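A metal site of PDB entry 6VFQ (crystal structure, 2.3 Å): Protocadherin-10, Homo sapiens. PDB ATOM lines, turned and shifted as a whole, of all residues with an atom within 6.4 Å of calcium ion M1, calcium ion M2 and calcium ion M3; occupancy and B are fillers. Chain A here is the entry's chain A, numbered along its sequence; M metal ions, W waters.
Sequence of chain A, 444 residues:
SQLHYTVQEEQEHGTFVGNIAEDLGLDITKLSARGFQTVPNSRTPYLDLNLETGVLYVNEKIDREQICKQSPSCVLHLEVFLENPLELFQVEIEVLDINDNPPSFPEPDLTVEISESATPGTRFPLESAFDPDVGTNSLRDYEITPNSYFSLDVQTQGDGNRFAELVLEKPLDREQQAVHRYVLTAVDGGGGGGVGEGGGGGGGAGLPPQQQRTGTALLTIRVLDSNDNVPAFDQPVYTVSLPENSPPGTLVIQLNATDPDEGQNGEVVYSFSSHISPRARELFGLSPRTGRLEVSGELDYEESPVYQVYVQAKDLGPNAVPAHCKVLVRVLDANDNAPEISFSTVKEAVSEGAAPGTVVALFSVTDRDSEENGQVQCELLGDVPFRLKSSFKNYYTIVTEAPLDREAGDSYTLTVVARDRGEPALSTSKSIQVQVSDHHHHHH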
ATOM      1  N   GLU A 244       2.223  -0.983 -11.927  1.00  0.00           N
ATOM      2  CA  GLU A 244       0.943  -1.648 -11.790  1.00  0.00           C
ATOM      3  C   GLU A 244       0.981  -2.566 -10.585  1.00  0.00           C
ATOM      4  O   GLU A 244       2.047  -2.982 -10.114  1.00  0.00           O
ATOM      5  CB  GLU A 244       0.586  -2.427 -13.067  1.00  0.00           C
ATOM      6  CG  GLU A 244       1.333  -3.725 -13.240  1.00  0.00           C
ATOM      7  CD  GLU A 244       0.877  -4.579 -14.432  1.00  0.00           C
ATOM      8  OE1 GLU A 244      -0.352  -4.742 -14.656  1.00  0.00           O
ATOM      9  OE2 GLU A 244       1.768  -5.106 -15.127  1.00  0.00           O
ATOM     10  N   ASN A 245      -0.185  -2.870 -10.062  1.00  0.00           N
ATOM     11  CA  ASN A 245      -0.304  -3.641  -8.824  1.00  0.00           C
ATOM     12  C   ASN A 245       0.293  -2.916  -7.605  1.00  0.00           C
ATOM     13  O   ASN A 245       0.502  -3.544  -6.555  1.00  0.00           O
ATOM     14  CB  ASN A 245       0.337  -5.029  -8.989  1.00  0.00           C
ATOM     15  CG  ASN A 245      -0.199  -5.775 -10.198  1.00  0.00           C
ATOM     16  OD1 ASN A 245      -1.405  -5.736 -10.477  1.00  0.00           O
ATOM     17  ND2 ASN A 245       0.678  -6.448 -10.924  1.00  0.00           N
ATOM     18  N   LEU A 299      -4.156  -0.953  -9.808  1.00  0.00           N
ATOM     19  CA  LEU A 299      -3.723  -0.413 -11.079  1.00  0.00           C
ATOM     20  C   LEU A 299      -3.299  -1.557 -11.982  1.00  0.00           C
ATOM     21  O   LEU A 299      -2.317  -2.256 -11.673  1.00  0.00           O
ATOM     22  CB  LEU A 299      -2.571   0.546 -10.873  1.00  0.00           C
ATOM     23  CG  LEU A 299      -2.921   1.747 -10.001  1.00  0.00           C
ATOM     24  CD1 LEU A 299      -1.688   2.601  -9.720  1.00  0.00           C
ATOM     25  CD2 LEU A 299      -3.991   2.587 -10.678  1.00  0.00           C
ATOM     26  N   ASP A 300      -4.013  -1.757 -13.081  1.00  0.00           N
ATOM     27  CA  ASP A 300      -3.730  -2.833 -14.032  1.00  0.00           C
ATOM     28  C   ASP A 300      -3.281  -2.225 -15.362  1.00  0.00           C
ATOM     29  O   ASP A 300      -4.093  -1.639 -16.084  1.00  0.00           O
ATOM     30  CB  ASP A 300      -4.945  -3.734 -14.227  1.00  0.00           C
ATOM     31  CG  ASP A 300      -4.712  -4.795 -15.287  1.00  0.00           C
ATOM     32  OD1 ASP A 300      -3.546  -5.001 -15.721  1.00  0.00           O
ATOM     33  OD2 ASP A 300      -5.692  -5.437 -15.690  1.00  0.00           O
ATOM     34  N   TYR A 301      -2.002  -2.386 -15.691  1.00  0.00           N
ATOM     35  CA  TYR A 301      -1.477  -1.899 -16.965  1.00  0.00           C
ATOM     36  C   TYR A 301      -2.262  -2.478 -18.144  1.00  0.00           C
ATOM     37  O   TYR A 301      -2.595  -1.760 -19.093  1.00  0.00           O
ATOM     38  CB  TYR A 301      -0.004  -2.269 -17.091  1.00  0.00           C
ATOM     39  CG  TYR A 301       0.629  -1.787 -18.356  1.00  0.00           C
ATOM     40  CD1 TYR A 301       0.609  -2.553 -19.512  1.00  0.00           C
ATOM     41  CD2 TYR A 301       1.247  -0.558 -18.398  1.00  0.00           C
ATOM     42  CE1 TYR A 301       1.206  -2.086 -20.696  1.00  0.00           C
ATOM     43  CE2 TYR A 301       1.835  -0.092 -19.545  1.00  0.00           C
ATOM     44  CZ  TYR A 301       1.809  -0.841 -20.691  1.00  0.00           C
ATOM     45  OH  TYR A 301       2.412  -0.325 -21.814  1.00  0.00           O
ATOM     46  N   GLU A 302      -2.558  -3.780 -18.107  1.00  0.00           N
ATOM     47  CA  GLU A 302      -3.258  -4.388 -19.215  1.00  0.00           C
ATOM     48  C   GLU A 302      -4.681  -3.870 -19.355  1.00  0.00           C
ATOM     49  O   GLU A 302      -5.340  -4.193 -20.349  1.00  0.00           O
ATOM     50  CB  GLU A 302      -3.249  -5.920 -19.081  1.00  0.00           C
ATOM     51  CG  GLU A 302      -1.889  -6.553 -19.376  1.00  0.00           C
ATOM     52  CD  GLU A 302      -0.849  -6.374 -18.264  1.00  0.00           C
ATOM     53  OE1 GLU A 302      -1.150  -6.657 -17.077  1.00  0.00           O
ATOM     54  OE2 GLU A 302       0.293  -5.961 -18.582  1.00  0.00           O
ATOM     55  N   GLU A 303      -5.168  -3.090 -18.397  1.00  0.00           N
ATOM     56  CA  GLU A 303      -6.448  -2.406 -18.510  1.00  0.00           C
ATOM     57  C   GLU A 303      -6.294  -0.998 -19.063  1.00  0.00           C
ATOM     58  O   GLU A 303      -7.060  -0.583 -19.937  1.00  0.00           O
ATOM     59  CB  GLU A 303      -7.129  -2.351 -17.146  1.00  0.00           C
ATOM     60  CG  GLU A 303      -8.493  -1.691 -17.149  1.00  0.00           C
ATOM     61  CD  GLU A 303      -9.063  -1.557 -15.753  1.00  0.00           C
ATOM     62  OE1 GLU A 303      -8.351  -1.903 -14.783  1.00  0.00           O
ATOM     63  OE2 GLU A 303     -10.227  -1.099 -15.621  1.00  0.00           O
ATOM     64  N   LEU A 332       3.092   1.509 -15.011  1.00  0.00           N
ATOM     65  CA  LEU A 332       4.245   0.788 -15.532  1.00  0.00           C
ATOM     66  C   LEU A 332       3.939  -0.700 -15.538  1.00  0.00           C
ATOM     67  O   LEU A 332       3.425  -1.237 -14.550  1.00  0.00           O
ATOM     68  CB  LEU A 332       5.486   1.073 -14.696  1.00  0.00           C
ATOM     69  CG  LEU A 332       5.877   2.536 -14.605  1.00  0.00           C
ATOM     70  CD1 LEU A 332       7.056   2.673 -13.664  1.00  0.00           C
ATOM     71  CD2 LEU A 332       6.233   3.077 -15.976  1.00  0.00           C
ATOM     72  N   ASP A 333       4.218  -1.351 -16.659  1.00  0.00           N
ATOM     73  CA  ASP A 333       3.891  -2.757 -16.824  1.00  0.00           C
ATOM     74  C   ASP A 333       4.812  -3.616 -15.963  1.00  0.00           C
ATOM     75  O   ASP A 333       6.020  -3.402 -15.928  1.00  0.00           O
ATOM     76  CB  ASP A 333       4.000  -3.125 -18.310  1.00  0.00           C
ATOM     77  CG  ASP A 333       3.910  -4.640 -18.587  1.00  0.00           C
ATOM     78  OD1 ASP A 333       2.892  -5.314 -18.256  1.00  0.00           O
ATOM     79  OD2 ASP A 333       4.887  -5.135 -19.189  1.00  0.00           O
ATOM     80  N   ALA A 334       4.215  -4.564 -15.245  1.00  0.00           N
ATOM     81  CA  ALA A 334       4.919  -5.631 -14.558  1.00  0.00           C
ATOM     82  C   ALA A 334       4.676  -6.975 -15.266  1.00  0.00           C
ATOM     83  O   ALA A 334       3.813  -7.103 -16.130  1.00  0.00           O
ATOM     84  CB  ALA A 334       4.451  -5.723 -13.100  1.00  0.00           C
ATOM     85  N   ASN A 335       5.426  -8.005 -14.848  1.00  0.00           N
ATOM     86  CA  ASN A 335       5.266  -9.340 -15.429  1.00  0.00           C
ATOM     87  C   ASN A 335       4.311 -10.135 -14.560  1.00  0.00           C
ATOM     88  O   ASN A 335       4.694 -10.972 -13.746  1.00  0.00           O
ATOM     89  CB  ASN A 335       6.611 -10.042 -15.584  1.00  0.00           C
ATOM     90  CG  ASN A 335       6.502 -11.327 -16.451  1.00  0.00           C
ATOM     91  OD1 ASN A 335       5.596 -11.479 -17.262  1.00  0.00           O
ATOM     92  ND2 ASN A 335       7.435 -12.257 -16.250  1.00  0.00           N
ATOM     93  N   ASP A 336       3.022  -9.883 -14.772  1.00  0.00           N
ATOM     94  CA  ASP A 336       1.970 -10.560 -14.027  1.00  0.00           C
ATOM     95  C   ASP A 336       1.084 -11.440 -14.898  1.00  0.00           C
ATOM     96  O   ASP A 336       0.031 -11.887 -14.420  1.00  0.00           O
ATOM     97  CB  ASP A 336       1.127  -9.531 -13.262  1.00  0.00           C
ATOM     98  CG  ASP A 336       0.583  -8.389 -14.139  1.00  0.00           C
ATOM     99  OD1 ASP A 336       1.030  -8.217 -15.304  1.00  0.00           O
ATOM    100  OD2 ASP A 336      -0.306  -7.664 -13.638  1.00  0.00           O
ATOM    101  N   ASN A 337       1.456 -11.726 -16.138  1.00  0.00           N
ATOM    102  CA  ASN A 337       0.753 -12.730 -16.931  1.00  0.00           C
ATOM    103  C   ASN A 337       1.730 -13.794 -17.431  1.00  0.00           C
ATOM    104  O   ASN A 337       2.795 -13.476 -17.971  1.00  0.00           O
ATOM    105  CB  ASN A 337       0.019 -12.091 -18.106  1.00  0.00           C
ATOM    106  CG  ASN A 337      -1.119 -11.203 -17.647  1.00  0.00           C
ATOM    107  OD1 ASN A 337      -2.238 -11.657 -17.427  1.00  0.00           O
ATOM    108  ND2 ASN A 337      -0.844  -9.922 -17.505  1.00  0.00           N
ATOM    109  N   ALA A 338       1.366 -14.987 -17.272  1.00  0.00           N
ATOM    110  CA  ALA A 338       2.188 -16.062 -17.779  1.00  0.00           C
ATOM    111  C   ALA A 338       1.824 -16.379 -19.228  1.00  0.00           C
ATOM    112  O   ALA A 338       0.680 -16.160 -19.641  1.00  0.00           O
ATOM    113  CB  ALA A 338       2.016 -17.310 -16.923  1.00  0.00           C
ATOM    114  N   PRO A 339       2.780 -16.882 -20.005  1.00  0.00           N
ATOM    115  CA  PRO A 339       2.477 -17.306 -21.387  1.00  0.00           C
ATOM    116  C   PRO A 339       1.313 -18.284 -21.472  1.00  0.00           C
ATOM    117  O   PRO A 339       1.083 -19.091 -20.568  1.00  0.00           O
ATOM    118  CB  PRO A 339       3.785 -17.980 -21.822  1.00  0.00           C
ATOM    119  CG  PRO A 339       4.842 -17.351 -20.987  1.00  0.00           C
ATOM    120  CD  PRO A 339       4.203 -16.996 -19.686  1.00  0.00           C
ATOM    121  N   ASP A 367       1.243 -13.930 -24.622  1.00  0.00           N
ATOM    122  CA  ASP A 367       1.523 -13.381 -23.294  1.00  0.00           C
ATOM    123  C   ASP A 367       0.917 -11.979 -23.210  1.00  0.00           C
ATOM    124  O   ASP A 367       1.284 -11.101 -23.999  1.00  0.00           O
ATOM    125  CB  ASP A 367       3.051 -13.344 -23.042  1.00  0.00           C
ATOM    126  CG  ASP A 367       3.408 -13.041 -21.575  1.00  0.00           C
ATOM    127  OD1 ASP A 367       2.919 -12.035 -21.015  1.00  0.00           O
ATOM    128  OD2 ASP A 367       4.197 -13.810 -20.985  1.00  0.00           O
ATOM    129  N   ARG A 368      -0.015 -11.774 -22.278  1.00  0.00           N
ATOM    130  CA  ARG A 368      -0.752 -10.511 -22.220  1.00  0.00           C
ATOM    131  C   ARG A 368       0.119  -9.315 -21.857  1.00  0.00           C
ATOM    132  O   ARG A 368      -0.347  -8.172 -21.971  1.00  0.00           O
ATOM    133  CB  ARG A 368      -1.906 -10.579 -21.207  1.00  0.00           C
ATOM    134  CG  ARG A 368      -2.941 -11.694 -21.454  1.00  0.00           C
ATOM    135  CD  ARG A 368      -4.397 -11.244 -21.252  1.00  0.00           C
ATOM    136  NE  ARG A 368      -4.607 -10.572 -19.971  1.00  0.00           N
ATOM    137  CZ  ARG A 368      -5.088  -9.337 -19.809  1.00  0.00           C
ATOM    138  NH1 ARG A 368      -5.441  -8.599 -20.859  1.00  0.00           N
ATOM    139  NH2 ARG A 368      -5.227  -8.841 -18.583  1.00  0.00           N
ATOM    140  N   ASP A 369       1.354  -9.551 -21.427  1.00  0.00           N
ATOM    141  CA  ASP A 369       2.247  -8.478 -21.032  1.00  0.00           C
ATOM    142  C   ASP A 369       2.878  -7.837 -22.278  1.00  0.00           C
ATOM    143  O   ASP A 369       2.595  -8.212 -23.416  1.00  0.00           O
ATOM    144  CB  ASP A 369       3.299  -9.005 -20.061  1.00  0.00           C
ATOM    145  CG  ASP A 369       2.697  -9.452 -18.736  1.00  0.00           C
ATOM    146  OD1 ASP A 369       1.833  -8.708 -18.195  1.00  0.00           O
ATOM    147  OD2 ASP A 369       3.057 -10.544 -18.234  1.00  0.00           O
ATOM    148  N   SER A 370       3.762  -6.868 -22.056  1.00  0.00           N
ATOM    149  CA  SER A 370       4.362  -6.067 -23.125  1.00  0.00           C
ATOM    150  C   SER A 370       5.881  -6.101 -22.980  1.00  0.00           C
ATOM    151  O   SER A 370       6.414  -6.384 -21.913  1.00  0.00           O
ATOM    152  CB  SER A 370       3.865  -4.615 -23.083  1.00  0.00           C
ATOM    153  OG  SER A 370       2.449  -4.538 -23.143  1.00  0.00           O
ATOM    154  N   GLU A 372       9.703  -7.181 -22.946  1.00  0.00           N
ATOM    155  CA  GLU A 372      10.268  -8.404 -22.397  1.00  0.00           C
ATOM    156  C   GLU A 372       9.253  -9.213 -21.617  1.00  0.00           C
ATOM    157  O   GLU A 372       9.292 -10.447 -21.626  1.00  0.00           O
ATOM    158  CB  GLU A 372      11.453  -8.073 -21.489  1.00  0.00           C
ATOM    159  CG  GLU A 372      12.679  -7.500 -22.190  1.00  0.00           C
ATOM    160  CD  GLU A 372      13.728  -7.018 -21.203  1.00  0.00           C
ATOM    161  OE1 GLU A 372      13.392  -6.840 -20.007  1.00  0.00           O
ATOM    162  OE2 GLU A 372      14.901  -6.820 -21.612  1.00  0.00           O
ATOM    163  N   ASN A 373       8.369  -8.553 -20.874  1.00  0.00           N
ATOM    164  CA  ASN A 373       7.423  -9.316 -20.071  1.00  0.00           C
ATOM    165  C   ASN A 373       6.485 -10.139 -20.945  1.00  0.00           C
ATOM    166  O   ASN A 373       5.862 -11.084 -20.441  1.00  0.00           O
ATOM    167  CB  ASN A 373       6.610  -8.394 -19.161  1.00  0.00           C
ATOM    168  CG  ASN A 373       7.490  -7.556 -18.243  1.00  0.00           C
ATOM    169  OD1 ASN A 373       8.431  -8.061 -17.620  1.00  0.00           O
ATOM    170  ND2 ASN A 373       7.178  -6.266 -18.156  1.00  0.00           N
ATOM    171  N   GLY A 374       6.360  -9.792 -22.227  1.00  0.00           N
ATOM    172  CA  GLY A 374       5.508 -10.499 -23.161  1.00  0.00           C
ATOM    173  C   GLY A 374       6.257 -11.276 -24.220  1.00  0.00           C
ATOM    174  O   GLY A 374       5.625 -11.794 -25.141  1.00  0.00           O
ATOM    175  N   GLN A 375       7.586 -11.376 -24.130  1.00  0.00           N
ATOM    176  CA  GLN A 375       8.408 -12.143 -25.048  1.00  0.00           C
ATOM    177  C   GLN A 375       8.545 -13.565 -24.530  1.00  0.00           C
ATOM    178  O   GLN A 375       8.925 -13.771 -23.375  1.00  0.00           O
ATOM    179  CB  GLN A 375       9.799 -11.521 -25.174  1.00  0.00           C
ATOM    180  CG  GLN A 375       9.900 -10.380 -26.132  1.00  0.00           C
ATOM    181  CD  GLN A 375      11.300  -9.776 -26.108  1.00  0.00           C
ATOM    182  OE1 GLN A 375      12.099 -10.072 -25.210  1.00  0.00           O
ATOM    183  NE2 GLN A 375      11.600  -8.934 -27.089  1.00  0.00           N
ATOM    184  N   ASP A 420       8.348 -16.590 -20.454  1.00  0.00           N
ATOM    185  CA  ASP A 420       8.588 -15.208 -20.842  1.00  0.00           C
ATOM    186  C   ASP A 420       9.917 -14.731 -20.244  1.00  0.00           C
ATOM    187  O   ASP A 420      10.556 -15.425 -19.463  1.00  0.00           O
ATOM    188  CB  ASP A 420       7.431 -14.271 -20.433  1.00  0.00           C
ATOM    189  CG  ASP A 420       7.242 -14.160 -18.933  1.00  0.00           C
ATOM    190  OD1 ASP A 420       8.238 -14.118 -18.192  1.00  0.00           O
ATOM    191  OD2 ASP A 420       6.077 -14.106 -18.491  1.00  0.00           O
ATOM    192  N   ARG A 421      10.284 -13.499 -20.580  1.00  0.00           N
ATOM    193  CA  ARG A 421      11.584 -12.925 -20.248  1.00  0.00           C
ATOM    194  C   ARG A 421      11.479 -11.751 -19.281  1.00  0.00           C
ATOM    195  O   ARG A 421      12.271 -10.809 -19.357  1.00  0.00           O
ATOM    196  CB  ARG A 421      12.301 -12.503 -21.530  1.00  0.00           C
ATOM    197  CG  ARG A 421      12.812 -13.706 -22.333  1.00  0.00           C
ATOM    198  CD  ARG A 421      13.719 -13.274 -23.451  1.00  0.00           C
ATOM    199  NE  ARG A 421      14.944 -12.628 -22.981  1.00  0.00           N
ATOM    200  CZ  ARG A 421      16.046 -13.275 -22.612  1.00  0.00           C
ATOM    201  NH1 ARG A 421      16.096 -14.601 -22.627  1.00  0.00           N
ATOM    202  NH2 ARG A 421      17.115 -12.583 -22.222  1.00  0.00           N
ATOM    203  N   GLY A 422      10.509 -11.804 -18.369  1.00  0.00           N
ATOM    204  CA  GLY A 422      10.419 -10.848 -17.281  1.00  0.00           C
ATOM    205  C   GLY A 422      11.241 -11.251 -16.063  1.00  0.00           C
ATOM    206  O   GLY A 422      11.910 -12.287 -16.050  1.00  0.00           O
ATOM    207  N   LEU A 426       8.005 -16.043 -15.825  1.00  0.00           N
ATOM    208  CA  LEU A 426       6.843 -16.896 -15.678  1.00  0.00           C
ATOM    209  C   LEU A 426       6.824 -17.876 -16.826  1.00  0.00           C
ATOM    210  O   LEU A 426       7.269 -17.573 -17.928  1.00  0.00           O
ATOM    211  CB  LEU A 426       5.559 -16.071 -15.666  1.00  0.00           C
ATOM    212  CG  LEU A 426       5.487 -15.158 -14.442  1.00  0.00           C
ATOM    213  CD1 LEU A 426       4.328 -14.215 -14.589  1.00  0.00           C
ATOM    214  CD2 LEU A 426       5.359 -15.994 -13.181  1.00  0.00           C
HETATM  215 CA    CA M   1       1.579  -6.693 -16.867  1.00  0.00          CA
HETATM  216 CA    CA M   2      -1.905  -6.590 -14.933  1.00  0.00          CA
HETATM  217 CA    CA M   3       4.429 -12.333 -19.048  1.00  0.00          CA
HETATM  218  O   HOH W   1      -3.229  -8.504 -15.529  1.00  0.00           O
HETATM  219  O   HOH W   2      -3.041  -6.035 -12.714  1.00  0.00           O
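The backbone carbonyl oxygen of Leu 426 is in hydrogen-bond range of the backbone NH of Asp 420, 2.9 Å away. N of Glu 244 sits at hydrogen-bond distance from O of Leu 332 (2.9 Å). ND2 of Asn 373 is in hydrogen-bond range of OD2 of Asp 333 (2.8 Å). OD1 of Asp 336 lies close to ND2 of Asn 337, 3.4 Å away. The side-chain carboxylate (OD2) of Asp 336 lies close to the side-chain amide nitrogen (ND2) of Asn 245, 3.1 Å away. The backbone NH (N) of Gly 422 is in hydrogen-bond range of the side-chain carboxylate (OD1) of Asp 420. OE1 of Glu 244 lies close to N of Tyr 301 (3.1 Å). The side-chain amide nitrogen (ND2) of Asn 337 sits close to the side-chain carboxylate (OE1) of Glu 302, 3.3 Å away.
Six residues have an atom within 4 Å of calcium ion M1: Glu 244, Glu 302, Asp 333, Ala 334, Asp 336 and Asp 369. The nearest printed residue that does not touch calcium ion M1 is Asn 337 (4.1 Å).
Within 4 Å of calcium ion M2: Glu 244, Asp 300, Glu 302 and Asp 336.
Of the 27 residues printed, 6 come within 4 Å of calcium ion M3.
Calcium ion M1 is bound by OD1 of Asp 336 (2.3 Å), OE2 of Glu 302 (2.3 Å), OD1 of Asp 333 (2.4 Å), OE2 of Glu 244 (2.4 Å), O of Ala 334 (2.4 Å), OD1 of Asp 369 (2.4 Å) and OE1 of Glu 302 (2.7 Å).
OE1 of Glu 302 is bound to calcium ion M2, 2.3 Å away. The side-chain carboxylate (OD2) of Asp 336 is bound to calcium ion M2 (2.3 Å). Water W1 is bound to calcium ion M2, at 2.4 Å. OD1 of Asp 300 is bound to calcium ion M2, 2.4 Å away. OE1 of Glu 244 is bound to calcium ion M2, at 2.4 Å. Calcium ion M2 is bound by water W2, 2.6 Å away. Calcium ion M2 has six donor atoms within binding distance.
O of Asn 337 is bound to calcium ion M3, at 2.3 Å. OD1 of Asn 335 is bound to calcium ion M3, 2.3 Å away. The backbone carbonyl oxygen (O) of Asn 373 binds calcium ion M3 (2.4 Å). The side-chain carboxylate (OD2) of Asp 369 is bound to calcium ion M3, 2.4 Å away. OD2 of Asp 367 is bound to calcium ion M3 (2.4 Å). Calcium ion M3 is bound by the side-chain carboxylate (OD2) of Asp 420, at 2.5 Å. OD1 of Asp 367 binds calcium ion M3 (2.5 Å). Calcium ion M3 has seven donor atoms within binding distance.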
